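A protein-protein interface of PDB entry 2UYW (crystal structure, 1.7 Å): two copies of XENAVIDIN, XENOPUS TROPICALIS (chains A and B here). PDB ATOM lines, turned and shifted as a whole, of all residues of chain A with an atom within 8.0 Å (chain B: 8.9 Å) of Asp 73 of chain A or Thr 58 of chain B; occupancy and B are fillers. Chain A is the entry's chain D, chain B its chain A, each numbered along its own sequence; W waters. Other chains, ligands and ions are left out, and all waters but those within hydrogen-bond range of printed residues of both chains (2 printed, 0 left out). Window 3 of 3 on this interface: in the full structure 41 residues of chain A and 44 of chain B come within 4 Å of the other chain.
Of the 17 printed residues of chain B, 9 touch a printed residue of chain A.
Hydrophobic or aromatic side chains of chain A within 4 Å of the printed part of chain B: His 68 and Ile 75.
Among the printed residues, no Asp or Glu carboxylate lies within 4 Å of a Lys or Arg side-chain nitrogen of the other chain.
Thr 42 of chain A touches none of the printed residues of chain B.
Phe 71 of chain A touches none of the printed residues of chain B.
Ser 72 of chain A touches just one residue of chain B: Lys 56.
Asp 73 of chain A touches three residues of chain B.
Printed residues of chain B within 4 Å of Ile 75 of chain A: Lys 56 (3.8 Å), Thr 62 (3.6 Å), Phe 63 (3.7 Å) and Thr 79 (3.5 Å).
Of the printed residues of chain B, Ser 100 of chain A touches Gln 81.
Thr 58 of chain B touches one residue of chain A.
Printed residues of chain A within 4 Å of Thr 79 of chain B: Ile 75 and Arg 99.
The nearest residue of chain A that does not touch Thr 58 of chain B is Ser 101 of chain A (5.4 Å).
O of Glu 103 of chain A lies within hydrogen-bond range of NZ of Lys 60 of chain B.
NZ of Lys 56 of chain B lies within hydrogen-bond range of O of Trp 69 of chain A (2.9 Å).
The backbone carbonyl oxygen of Asp 73 of chain A lies within hydrogen-bond range of the side-chain hydroxyl of Thr 62 of chain B, 2.7 Å away.
NE2 of Gln 81 of chain B is in hydrogen-bond range of OG of Ser 101 of chain A, at 3.4 Å.
The backbone carbonyl oxygen (O) of Ser 74 of chain A sits at hydrogen-bond distance from the side-chain amino group (NZ) of Lys 56 of chain B.
The side-chain amide oxygen (OE1) of Gln 81 of chain B lies within hydrogen-bond range of the backbone NH (N) of Gln 102 of chain A (2.8 Å).
OE1 of Gln 81 of chain B is in hydrogen-bond range of NH2 of Arg 99 of chain A (2.9 Å).
A ring nitrogen (ND1) of His 68 of chain A sits at hydrogen-bond distance from the side-chain amino group (NZ) of Lys 56 of chain B, 2.9 Å away.
No position is printed for both chains.
Of the 21 pairs that touch across the chains among the printed residues, none has its exchanged pair printed and touching as well.
Water W1 lies within hydrogen-bond range of the backbone carbonyl oxygen of Lys 60 of chain B (2.7 Å), the side-chain hydroxyl of Ser 101 of chain A (2.9 Å), the side-chain hydroxyl of Thr 58 of chain B (3.2 Å) and the backbone NH of Thr 62 of chain B (3.4 Å).
Water W2 lies within hydrogen-bond range of O of Thr 79 of chain B (2.9 Å) and NH1 of Arg 99 of chain A (3.0 Å).
His 68 of chain A touches Gln 55 of chain B.
Ser 72 of chain A touches Lys 56 of chain B (O to CE, 3.2 Å).
Thr 58 of chain B touches Asp 73 of chain A.
CD1 of Ile 75 of chain A touches NZ of Lys 56 of chain B (3.8 Å).
Ile 75 of chain A touches Thr 62 of chain B.
N of Phe 63 of chain B touches CG1 of Ile 75 of chain A (3.7 Å).
Ile 75 of chain A touches Thr 79 of chain B (CG2 to OG1, 3.5 Å).
CG of Arg 99 of chain A touches CG2 of Thr 62 of chain B, 3.7 Å away.
O of Gly 80 of chain B touches CG of Arg 99 of chain A, at 3.5 Å.
Gln 81 of chain B touches Ser 100 of chain A.
The backbone carbonyl oxygen (O) of Cys 6 of chain B sits at hydrogen-bond distance from the side-chain amide nitrogen (NE2) of Gln 55 of chain B, at 3.5 Å.
The backbone carbonyl oxygen of Ile 75 of chain A is in hydrogen-bond range of the backbone NH of Arg 99 of chain A.
The backbone carbonyl oxygen (O) of Gly 29 of chain B is in hydrogen-bond range of the backbone NH (N) of Gln 55 of chain B (2.8 Å).
N of Phe 63 of chain B sits at hydrogen-bond distance from O of Gly 80 of chain B (3.0 Å).
N of Lys 56 of chain B lies within hydrogen-bond range of O of Thr 62 of chain B (2.9 Å).
NE1 of Trp 69 of chain A lies within hydrogen-bond range of OG1 of Thr 76 of chain A (2.9 Å).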
ATOM      1  N   THR A  42     -19.041 -12.172  12.473  1.00  0.00           N
ATOM      2  CA  THR A  42     -18.893 -11.283  13.659  1.00  0.00           C
ATOM      3  C   THR A  42     -19.062 -12.009  14.995  1.00  0.00           C
ATOM      4  O   THR A  42     -19.211 -13.231  15.040  1.00  0.00           O
ATOM      5  CB  THR A  42     -19.867 -10.068  13.633  1.00  0.00           C
ATOM      6  OG1 THR A  42     -21.229 -10.514  13.761  1.00  0.00           O
ATOM      7  CG2 THR A  42     -19.676  -9.231  12.369  1.00  0.00           C
ATOM      8  N   HIS A  68     -31.822 -16.543   5.519  1.00  0.00           N
ATOM      9  CA  HIS A  68     -32.051 -15.124   5.917  1.00  0.00           C
ATOM     10  C   HIS A  68     -31.522 -14.963   7.339  1.00  0.00           C
ATOM     11  O   HIS A  68     -32.272 -15.091   8.296  1.00  0.00           O
ATOM     12  CB  HIS A  68     -33.568 -14.899   5.860  1.00  0.00           C
ATOM     13  CG  HIS A  68     -34.027 -13.497   6.134  1.00  0.00           C
ATOM     14  ND1 HIS A  68     -33.183 -12.414   6.215  1.00  0.00           N
ATOM     15  CD2 HIS A  68     -35.283 -13.014   6.316  1.00  0.00           C
ATOM     16  CE1 HIS A  68     -33.896 -11.326   6.471  1.00  0.00           C
ATOM     17  NE2 HIS A  68     -35.176 -11.658   6.502  1.00  0.00           N
ATOM     18  N   TRP A  69     -30.217 -14.712   7.479  1.00  0.00           N
ATOM     19  CA  TRP A  69     -29.581 -14.750   8.798  1.00  0.00           C
ATOM     20  C   TRP A  69     -30.310 -13.808   9.784  1.00  0.00           C
ATOM     21  O   TRP A  69     -30.537 -12.626   9.483  1.00  0.00           O
ATOM     22  CB  TRP A  69     -28.101 -14.363   8.694  1.00  0.00           C
ATOM     23  CG  TRP A  69     -27.328 -15.301   7.798  1.00  0.00           C
ATOM     24  CD1 TRP A  69     -26.832 -15.024   6.562  1.00  0.00           C
ATOM     25  CD2 TRP A  69     -27.014 -16.688   8.069  1.00  0.00           C
ATOM     26  NE1 TRP A  69     -26.179 -16.155   6.052  1.00  0.00           N
ATOM     27  CE2 TRP A  69     -26.291 -17.180   6.955  1.00  0.00           C
ATOM     28  CE3 TRP A  69     -27.263 -17.549   9.159  1.00  0.00           C
ATOM     29  CZ2 TRP A  69     -25.802 -18.508   6.889  1.00  0.00           C
ATOM     30  CZ3 TRP A  69     -26.796 -18.867   9.082  1.00  0.00           C
ATOM     31  CH2 TRP A  69     -26.075 -19.329   7.941  1.00  0.00           C
ATOM     32  N   ALA A  70     -30.648 -14.333  10.961  1.00  0.00           N
ATOM     33  CA  ALA A  70     -31.454 -13.589  11.943  1.00  0.00           C
ATOM     34  C   ALA A  70     -30.632 -12.650  12.822  1.00  0.00           C
ATOM     35  O   ALA A  70     -31.197 -11.893  13.622  1.00  0.00           O
ATOM     36  CB  ALA A  70     -32.262 -14.565  12.819  1.00  0.00           C
ATOM     37  N   PHE A  71     -29.302 -12.692  12.686  1.00  0.00           N
ATOM     38  CA  PHE A  71     -28.427 -12.025  13.643  1.00  0.00           C
ATOM     39  C   PHE A  71     -27.382 -11.134  12.970  1.00  0.00           C
ATOM     40  O   PHE A  71     -26.477 -10.597  13.652  1.00  0.00           O
ATOM     41  CB  PHE A  71     -27.714 -13.078  14.504  1.00  0.00           C
ATOM     42  CG  PHE A  71     -26.931 -14.072  13.685  1.00  0.00           C
ATOM     43  CD1 PHE A  71     -25.585 -13.847  13.379  1.00  0.00           C
ATOM     44  CD2 PHE A  71     -27.545 -15.224  13.197  1.00  0.00           C
ATOM     45  CE1 PHE A  71     -24.878 -14.767  12.594  1.00  0.00           C
ATOM     46  CE2 PHE A  71     -26.852 -16.138  12.434  1.00  0.00           C
ATOM     47  CZ  PHE A  71     -25.507 -15.922  12.129  1.00  0.00           C
ATOM     48  N   SER A  72     -27.495 -10.997  11.644  1.00  0.00           N
ATOM     49  CA  SER A  72     -26.618 -10.114  10.863  1.00  0.00           C
ATOM     50  C   SER A  72     -27.360  -9.619   9.621  1.00  0.00           C
ATOM     51  O   SER A  72     -28.461 -10.072   9.341  1.00  0.00           O
ATOM     52  CB  SER A  72     -25.341 -10.849  10.434  1.00  0.00           C
ATOM     53  OG  SER A  72     -25.631 -11.668   9.309  1.00  0.00           O
ATOM     54  N   ASP A  73     -26.742  -8.704   8.876  1.00  0.00           N
ATOM     55  CA  ASP A  73     -27.366  -8.177   7.654  1.00  0.00           C
ATOM     56  C   ASP A  73     -26.915  -8.949   6.402  1.00  0.00           C
ATOM     57  O   ASP A  73     -27.117  -8.495   5.282  1.00  0.00           O
ATOM     58  CB  ASP A  73     -27.091  -6.655   7.488  1.00  0.00           C
ATOM     59  CG  ASP A  73     -27.832  -5.786   8.516  1.00  0.00           C
ATOM     60  OD1 ASP A  73     -28.902  -6.170   9.060  1.00  0.00           O
ATOM     61  OD2 ASP A  73     -27.344  -4.664   8.766  1.00  0.00           O
ATOM     62  N   SER A  74     -26.338 -10.136   6.604  1.00  0.00           N
ATOM     63  CA  SER A  74     -25.847 -10.997   5.500  1.00  0.00           C
ATOM     64  C   SER A  74     -26.948 -11.887   4.944  1.00  0.00           C
ATOM     65  O   SER A  74     -28.017 -12.054   5.558  1.00  0.00           O
ATOM     66  CB  SER A  74     -24.693 -11.884   5.997  1.00  0.00           C
ATOM     67  OG  SER A  74     -23.634 -11.075   6.467  1.00  0.00           O
ATOM     68  N   ILE A  75     -26.699 -12.448   3.766  1.00  0.00           N
ATOM     69  CA  ILE A  75     -27.537 -13.492   3.181  1.00  0.00           C
ATOM     70  C   ILE A  75     -26.559 -14.554   2.632  1.00  0.00           C
ATOM     71  O   ILE A  75     -25.492 -14.195   2.107  1.00  0.00           O
ATOM     72  CB  ILE A  75     -28.340 -12.934   1.975  1.00  0.00           C
ATOM     73  CG1 ILE A  75     -29.417 -11.935   2.436  1.00  0.00           C
ATOM     74  CG2 ILE A  75     -28.961 -14.092   1.147  1.00  0.00           C
ATOM     75  CD1 ILE A  75     -30.654 -12.557   3.212  1.00  0.00           C
ATOM     76  N   THR A  76     -26.907 -15.834   2.745  1.00  0.00           N
ATOM     77  CA  THR A  76     -26.121 -16.882   2.062  1.00  0.00           C
ATOM     78  C   THR A  76     -27.061 -17.706   1.195  1.00  0.00           C
ATOM     79  O   THR A  76     -28.205 -17.953   1.596  1.00  0.00           O
ATOM     80  CB  THR A  76     -25.371 -17.816   3.054  1.00  0.00           C
ATOM     81  OG1 THR A  76     -24.514 -17.036   3.906  1.00  0.00           O
ATOM     82  CG2 THR A  76     -24.535 -18.873   2.273  1.00  0.00           C
ATOM     83  N   LEU A  98     -21.819 -16.090   0.136  1.00  0.00           N
ATOM     84  CA  LEU A  98     -22.189 -15.341   1.338  1.00  0.00           C
ATOM     85  C   LEU A  98     -22.063 -13.874   1.009  1.00  0.00           C
ATOM     86  O   LEU A  98     -20.953 -13.367   0.743  1.00  0.00           O
ATOM     87  CB  LEU A  98     -21.260 -15.698   2.491  1.00  0.00           C
ATOM     88  CG  LEU A  98     -21.180 -14.826   3.768  1.00  0.00           C
ATOM     89  CD1 LEU A  98     -22.517 -14.514   4.353  1.00  0.00           C
ATOM     90  CD2 LEU A  98     -20.238 -15.474   4.839  1.00  0.00           C
ATOM     91  N   ARG A  99     -23.199 -13.199   0.974  1.00  0.00           N
ATOM     92  CA  ARG A  99     -23.202 -11.788   0.742  1.00  0.00           C
ATOM     93  C   ARG A  99     -23.198 -11.025   2.074  1.00  0.00           C
ATOM     94  O   ARG A  99     -24.098 -11.201   2.905  1.00  0.00           O
ATOM     95  CB  ARG A  99     -24.459 -11.418  -0.074  1.00  0.00           C
ATOM     96  CG  ARG A  99     -24.630  -9.888  -0.248  1.00  0.00           C
ATOM     97  CD  ARG A  99     -23.617  -9.356  -1.280  1.00  0.00           C
ATOM     98  NE  ARG A  99     -23.299  -7.926  -1.082  1.00  0.00           N
ATOM     99  CZ  ARG A  99     -22.904  -7.136  -2.076  1.00  0.00           C
ATOM    100  NH1 ARG A  99     -22.818  -7.631  -3.313  1.00  0.00           N
ATOM    101  NH2 ARG A  99     -22.594  -5.864  -1.850  1.00  0.00           N
ATOM    102  N   SER A 100     -22.212 -10.143   2.249  1.00  0.00           N
ATOM    103  CA  SER A 100     -22.208  -9.260   3.403  1.00  0.00           C
ATOM    104  C   SER A 100     -22.706  -7.879   2.978  1.00  0.00           C
ATOM    105  O   SER A 100     -22.540  -7.458   1.819  1.00  0.00           O
ATOM    106  CB  SER A 100     -20.814  -9.176   4.017  1.00  0.00           C
ATOM    107  OG  SER A 100     -19.856  -8.907   3.018  1.00  0.00           O
ATOM    108  N   SER A 101     -23.345  -7.195   3.913  1.00  0.00           N
ATOM    109  CA  SER A 101     -23.874  -5.880   3.641  1.00  0.00           C
ATOM    110  C   SER A 101     -22.780  -4.797   3.640  1.00  0.00           C
ATOM    111  O   SER A 101     -22.077  -4.568   4.654  1.00  0.00           O
ATOM    112  CB  SER A 101     -24.958  -5.568   4.665  1.00  0.00           C
ATOM    113  OG  SER A 101     -25.434  -4.244   4.480  1.00  0.00           O
ATOM    114  N   GLN A 102     -22.647  -4.121   2.502  1.00  0.00           N
ATOM    115  CA  GLN A 102     -21.695  -3.009   2.386  1.00  0.00           C
ATOM    116  C   GLN A 102     -22.342  -1.639   2.579  1.00  0.00           C
ATOM    117  O   GLN A 102     -23.524  -1.441   2.295  1.00  0.00           O
ATOM    118  CB  GLN A 102     -20.959  -3.082   1.045  1.00  0.00           C
ATOM    119  CG  GLN A 102     -20.231  -4.427   0.825  1.00  0.00           C
ATOM    120  CD  GLN A 102     -19.310  -4.770   1.971  1.00  0.00           C
ATOM    121  OE1 GLN A 102     -18.464  -3.963   2.364  1.00  0.00           O
ATOM    122  NE2 GLN A 102     -19.497  -5.962   2.545  1.00  0.00           N
ATOM    123  N   GLU A 103     -21.561  -0.697   3.097  1.00  0.00           N
ATOM    124  CA  GLU A 103     -22.090   0.624   3.421  1.00  0.00           C
ATOM    125  C   GLU A 103     -22.347   1.412   2.152  1.00  0.00           C
ATOM    126  O   GLU A 103     -23.265   2.251   2.086  1.00  0.00           O
ATOM    127  CB  GLU A 103     -21.118   1.381   4.324  1.00  0.00           C
ATOM    128  CG  GLU A 103     -20.337   0.485   5.302  1.00  0.00           C
ATOM    129  CD  GLU A 103     -20.825   0.584   6.745  1.00  0.00           C
ATOM    130  OE1 GLU A 103     -20.014   1.009   7.606  1.00  0.00           O
ATOM    131  OE2 GLU A 103     -22.004   0.243   7.014  1.00  0.00           O
ATOM    132  N   LYS B   5     -36.146   3.122  -2.249  1.00  0.00           N
ATOM    133  CA  LYS B   5     -35.417   2.720  -1.056  1.00  0.00           C
ATOM    134  C   LYS B   5     -35.193   1.211  -1.072  1.00  0.00           C
ATOM    135  O   LYS B   5     -35.202   0.560  -0.015  1.00  0.00           O
ATOM    136  CB  LYS B   5     -36.224   3.085   0.197  1.00  0.00           C
ATOM    137  CG  LYS B   5     -36.452   4.586   0.407  1.00  0.00           C
ATOM    138  CD  LYS B   5     -35.746   5.129   1.637  1.00  0.00           C
ATOM    139  CE  LYS B   5     -34.230   5.051   1.534  1.00  0.00           C
ATOM    140  NZ  LYS B   5     -33.598   5.589   2.777  1.00  0.00           N
ATOM    141  N   CYS B   6     -35.033   0.669  -2.282  1.00  0.00           N
ATOM    142  CA  CYS B   6     -34.657  -0.725  -2.501  1.00  0.00           C
ATOM    143  C   CYS B   6     -35.624  -1.785  -1.978  1.00  0.00           C
ATOM    144  O   CYS B   6     -35.211  -2.874  -1.561  1.00  0.00           O
ATOM    145  CB  CYS B   6     -33.250  -0.955  -1.980  1.00  0.00           C
ATOM    146  SG  CYS B   6     -31.996  -0.251  -3.068  1.00  0.00           S
ATOM    147  N   ASN B   7     -36.916  -1.474  -2.009  1.00  0.00           N
ATOM    148  CA  ASN B   7     -37.932  -2.508  -1.825  1.00  0.00           C
ATOM    149  C   ASN B   7     -37.997  -3.297  -3.138  1.00  0.00           C
ATOM    150  O   ASN B   7     -38.267  -2.715  -4.193  1.00  0.00           O
ATOM    151  CB  ASN B   7     -39.277  -1.878  -1.470  1.00  0.00           C
ATOM    152  CG  ASN B   7     -40.203  -2.849  -0.749  1.00  0.00           C
ATOM    153  OD1 ASN B   7     -40.548  -3.908  -1.278  1.00  0.00           O
ATOM    154  ND2 ASN B   7     -40.627  -2.477   0.467  1.00  0.00           N
ATOM    155  N   GLY B  29     -39.447 -10.280   5.179  1.00  0.00           N
ATOM    156  CA  GLY B  29     -38.508 -10.126   4.046  1.00  0.00           C
ATOM    157  C   GLY B  29     -38.641 -11.182   2.955  1.00  0.00           C
ATOM    158  O   GLY B  29     -37.920 -11.116   1.955  1.00  0.00           O
ATOM    159  N   GLN B  55     -35.209 -10.734   1.244  1.00  0.00           N
ATOM    160  CA  GLN B  55     -34.407  -9.535   1.342  1.00  0.00           C
ATOM    161  C   GLN B  55     -34.332  -9.051   2.783  1.00  0.00           C
ATOM    162  O   GLN B  55     -35.280  -9.225   3.583  1.00  0.00           O
ATOM    163  CB  GLN B  55     -34.967  -8.435   0.436  1.00  0.00           C
ATOM    164  CG  GLN B  55     -36.233  -7.775   0.953  1.00  0.00           C
ATOM    165  CD  GLN B  55     -36.452  -6.414   0.306  1.00  0.00           C
ATOM    166  OE1 GLN B  55     -37.204  -6.305  -0.658  1.00  0.00           O
ATOM    167  NE2 GLN B  55     -35.767  -5.373   0.815  1.00  0.00           N
ATOM    168  N   LYS B  56     -33.209  -8.412   3.094  1.00  0.00           N
ATOM    169  CA  LYS B  56     -33.072  -7.653   4.330  1.00  0.00           C
ATOM    170  C   LYS B  56     -33.997  -6.439   4.367  1.00  0.00           C
ATOM    171  O   LYS B  56     -34.432  -5.951   3.317  1.00  0.00           O
ATOM    172  CB  LYS B  56     -31.609  -7.192   4.485  1.00  0.00           C
ATOM    173  CG  LYS B  56     -30.836  -7.857   5.636  1.00  0.00           C
ATOM    174  CD  LYS B  56     -30.816  -9.379   5.530  1.00  0.00           C
ATOM    175  CE  LYS B  56     -30.573 -10.014   6.901  1.00  0.00           C
ATOM    176  NZ  LYS B  56     -30.496 -11.529   6.822  1.00  0.00           N
ATOM    177  N   LEU B  57     -34.291  -5.945   5.575  1.00  0.00           N
ATOM    178  CA  LEU B  57     -35.263  -4.864   5.742  1.00  0.00           C
ATOM    179  C   LEU B  57     -34.590  -3.537   6.024  1.00  0.00           C
ATOM    180  O   LEU B  57     -35.246  -2.591   6.413  1.00  0.00           O
ATOM    181  CB  LEU B  57     -36.223  -5.183   6.891  1.00  0.00           C
ATOM    182  CG  LEU B  57     -37.039  -6.483   6.795  1.00  0.00           C
ATOM    183  CD1 LEU B  57     -37.996  -6.574   7.992  1.00  0.00           C
ATOM    184  CD2 LEU B  57     -37.812  -6.540   5.476  1.00  0.00           C
ATOM    185  N   THR B  58     -33.277  -3.496   5.830  1.00  0.00           N
ATOM    186  CA  THR B  58     -32.448  -2.320   6.121  1.00  0.00           C
ATOM    187  C   THR B  58     -32.235  -1.463   4.860  1.00  0.00           C
ATOM    188  O   THR B  58     -32.605  -1.885   3.760  1.00  0.00           O
ATOM    189  CB  THR B  58     -31.080  -2.781   6.650  1.00  0.00           C
ATOM    190  OG1 THR B  58     -30.611  -3.837   5.832  1.00  0.00           O
ATOM    191  CG2 THR B  58     -31.201  -3.310   8.074  1.00  0.00           C
ATOM    192  N   GLU B  59     -31.705  -0.238   5.039  1.00  0.00           N
ATOM    193  CA  GLU B  59     -31.272   0.595   3.916  1.00  0.00           C
ATOM    194  C   GLU B  59     -30.205  -0.178   3.086  1.00  0.00           C
ATOM    195  O   GLU B  59     -29.299  -0.829   3.650  1.00  0.00           O
ATOM    196  CB  GLU B  59     -30.756   1.986   4.396  1.00  0.00           C
ATOM    197  CG  GLU B  59     -30.788   2.210   5.950  1.00  0.00           C
ATOM    198  CD  GLU B  59     -30.569   3.690   6.354  1.00  0.00           C
ATOM    199  OE1 GLU B  59     -30.184   3.947   7.532  1.00  0.00           O
ATOM    200  OE2 GLU B  59     -30.773   4.594   5.500  1.00  0.00           O
ATOM    201  N   LYS B  60     -30.339  -0.116   1.757  1.00  0.00           N
ATOM    202  CA  LYS B  60     -29.463  -0.831   0.805  1.00  0.00           C
ATOM    203  C   LYS B  60     -29.453  -2.368   1.066  1.00  0.00           C
ATOM    204  O   LYS B  60     -28.422  -2.963   1.411  1.00  0.00           O
ATOM    205  CB  LYS B  60     -28.035  -0.260   0.815  1.00  0.00           C
ATOM    206  CG  LYS B  60     -27.951   1.251   0.468  1.00  0.00           C
ATOM    207  CD  LYS B  60     -26.665   1.857   0.988  1.00  0.00           C
ATOM    208  CE  LYS B  60     -26.685   1.995   2.502  1.00  0.00           C
ATOM    209  NZ  LYS B  60     -25.751   3.053   2.957  1.00  0.00           N
ATOM    210  N   PRO B  61     -30.614  -3.011   0.912  1.00  0.00           N
ATOM    211  CA  PRO B  61     -30.731  -4.388   1.397  1.00  0.00           C
ATOM    212  C   PRO B  61     -29.927  -5.423   0.621  1.00  0.00           C
ATOM    213  O   PRO B  61     -29.885  -5.389  -0.612  1.00  0.00           O
ATOM    214  CB  PRO B  61     -32.209  -4.697   1.204  1.00  0.00           C
ATOM    215  CG  PRO B  61     -32.628  -3.797   0.074  1.00  0.00           C
ATOM    216  CD  PRO B  61     -31.878  -2.523   0.337  1.00  0.00           C
ATOM    217  N   THR B  62     -29.331  -6.353   1.359  1.00  0.00           N
ATOM    218  CA  THR B  62     -28.872  -7.608   0.766  1.00  0.00           C
ATOM    219  C   THR B  62     -30.087  -8.516   0.497  1.00  0.00           C
ATOM    220  O   THR B  62     -31.203  -8.308   1.040  1.00  0.00           O
ATOM    221  CB  THR B  62     -27.891  -8.326   1.718  1.00  0.00           C
ATOM    222  OG1 THR B  62     -28.528  -8.462   3.006  1.00  0.00           O
ATOM    223  CG2 THR B  62     -26.610  -7.522   1.871  1.00  0.00           C
ATOM    224  N   PHE B  63     -29.892  -9.540  -0.329  1.00  0.00           N
ATOM    225  CA  PHE B  63     -31.003 -10.433  -0.674  1.00  0.00           C
ATOM    226  C   PHE B  63     -30.416 -11.668  -1.338  1.00  0.00           C
ATOM    227  O   PHE B  63     -29.231 -11.706  -1.723  1.00  0.00           O
ATOM    228  CB  PHE B  63     -32.019  -9.750  -1.641  1.00  0.00           C
ATOM    229  CG  PHE B  63     -31.374  -9.309  -2.937  1.00  0.00           C
ATOM    230  CD1 PHE B  63     -31.248 -10.197  -4.007  1.00  0.00           C
ATOM    231  CD2 PHE B  63     -30.881  -8.016  -3.059  1.00  0.00           C
ATOM    232  CE1 PHE B  63     -30.570  -9.788  -5.190  1.00  0.00           C
ATOM    233  CE2 PHE B  63     -30.215  -7.605  -4.234  1.00  0.00           C
ATOM    234  CZ  PHE B  63     -30.090  -8.485  -5.295  1.00  0.00           C
ATOM    235  N   THR B  79     -27.190 -14.040  -5.084  1.00  0.00           N
ATOM    236  CA  THR B  79     -27.231 -13.188  -3.894  1.00  0.00           C
ATOM    237  C   THR B  79     -26.596 -11.864  -4.241  1.00  0.00           C
ATOM    238  O   THR B  79     -25.658 -11.806  -5.057  1.00  0.00           O
ATOM    239  CB  THR B  79     -26.544 -13.876  -2.657  1.00  0.00           C
ATOM    240  OG1 THR B  79     -26.792 -13.112  -1.469  1.00  0.00           O
ATOM    241  CG2 THR B  79     -25.029 -14.093  -2.866  1.00  0.00           C
ATOM    242  N   GLY B  80     -27.028 -10.804  -3.582  1.00  0.00           N
ATOM    243  CA  GLY B  80     -26.537  -9.500  -3.967  1.00  0.00           C
ATOM    244  C   GLY B  80     -26.994  -8.412  -3.028  1.00  0.00           C
ATOM    245  O   GLY B  80     -27.486  -8.687  -1.937  1.00  0.00           O
ATOM    246  N   GLN B  81     -26.793  -7.173  -3.443  1.00  0.00           N
ATOM    247  CA  GLN B  81     -27.194  -6.034  -2.633  1.00  0.00           C
ATOM    248  C   GLN B  81     -27.705  -4.932  -3.556  1.00  0.00           C
ATOM    249  O   GLN B  81     -27.148  -4.718  -4.652  1.00  0.00           O
ATOM    250  CB  GLN B  81     -26.025  -5.545  -1.760  1.00  0.00           C
ATOM    251  CG  GLN B  81     -26.407  -4.442  -0.768  1.00  0.00           C
ATOM    252  CD  GLN B  81     -25.329  -4.104   0.249  1.00  0.00           C
ATOM    253  OE1 GLN B  81     -24.181  -4.561   0.183  1.00  0.00           O
ATOM    254  NE2 GLN B  81     -25.688  -3.238   1.191  1.00  0.00           N
ATOM    255  N   CYS B  82     -28.752  -4.240  -3.097  1.00  0.00           N
ATOM    256  CA  CYS B  82     -29.374  -3.141  -3.821  1.00  0.00           C
ATOM    257  C   CYS B  82     -28.740  -1.848  -3.361  1.00  0.00           C
ATOM    258  O   CYS B  82     -28.585  -1.595  -2.168  1.00  0.00           O
ATOM    259  CB  CYS B  82     -30.889  -3.088  -3.547  1.00  0.00           C
ATOM    260  SG  CYS B  82     -31.748  -1.770  -4.444  1.00  0.00           S
HETATM  261  O   HOH W   1     -28.207  -4.263   3.785  1.00  0.00           O
HETATM  262  O   HOH W   2     -23.223 -10.188  -4.776  1.00  0.00           O
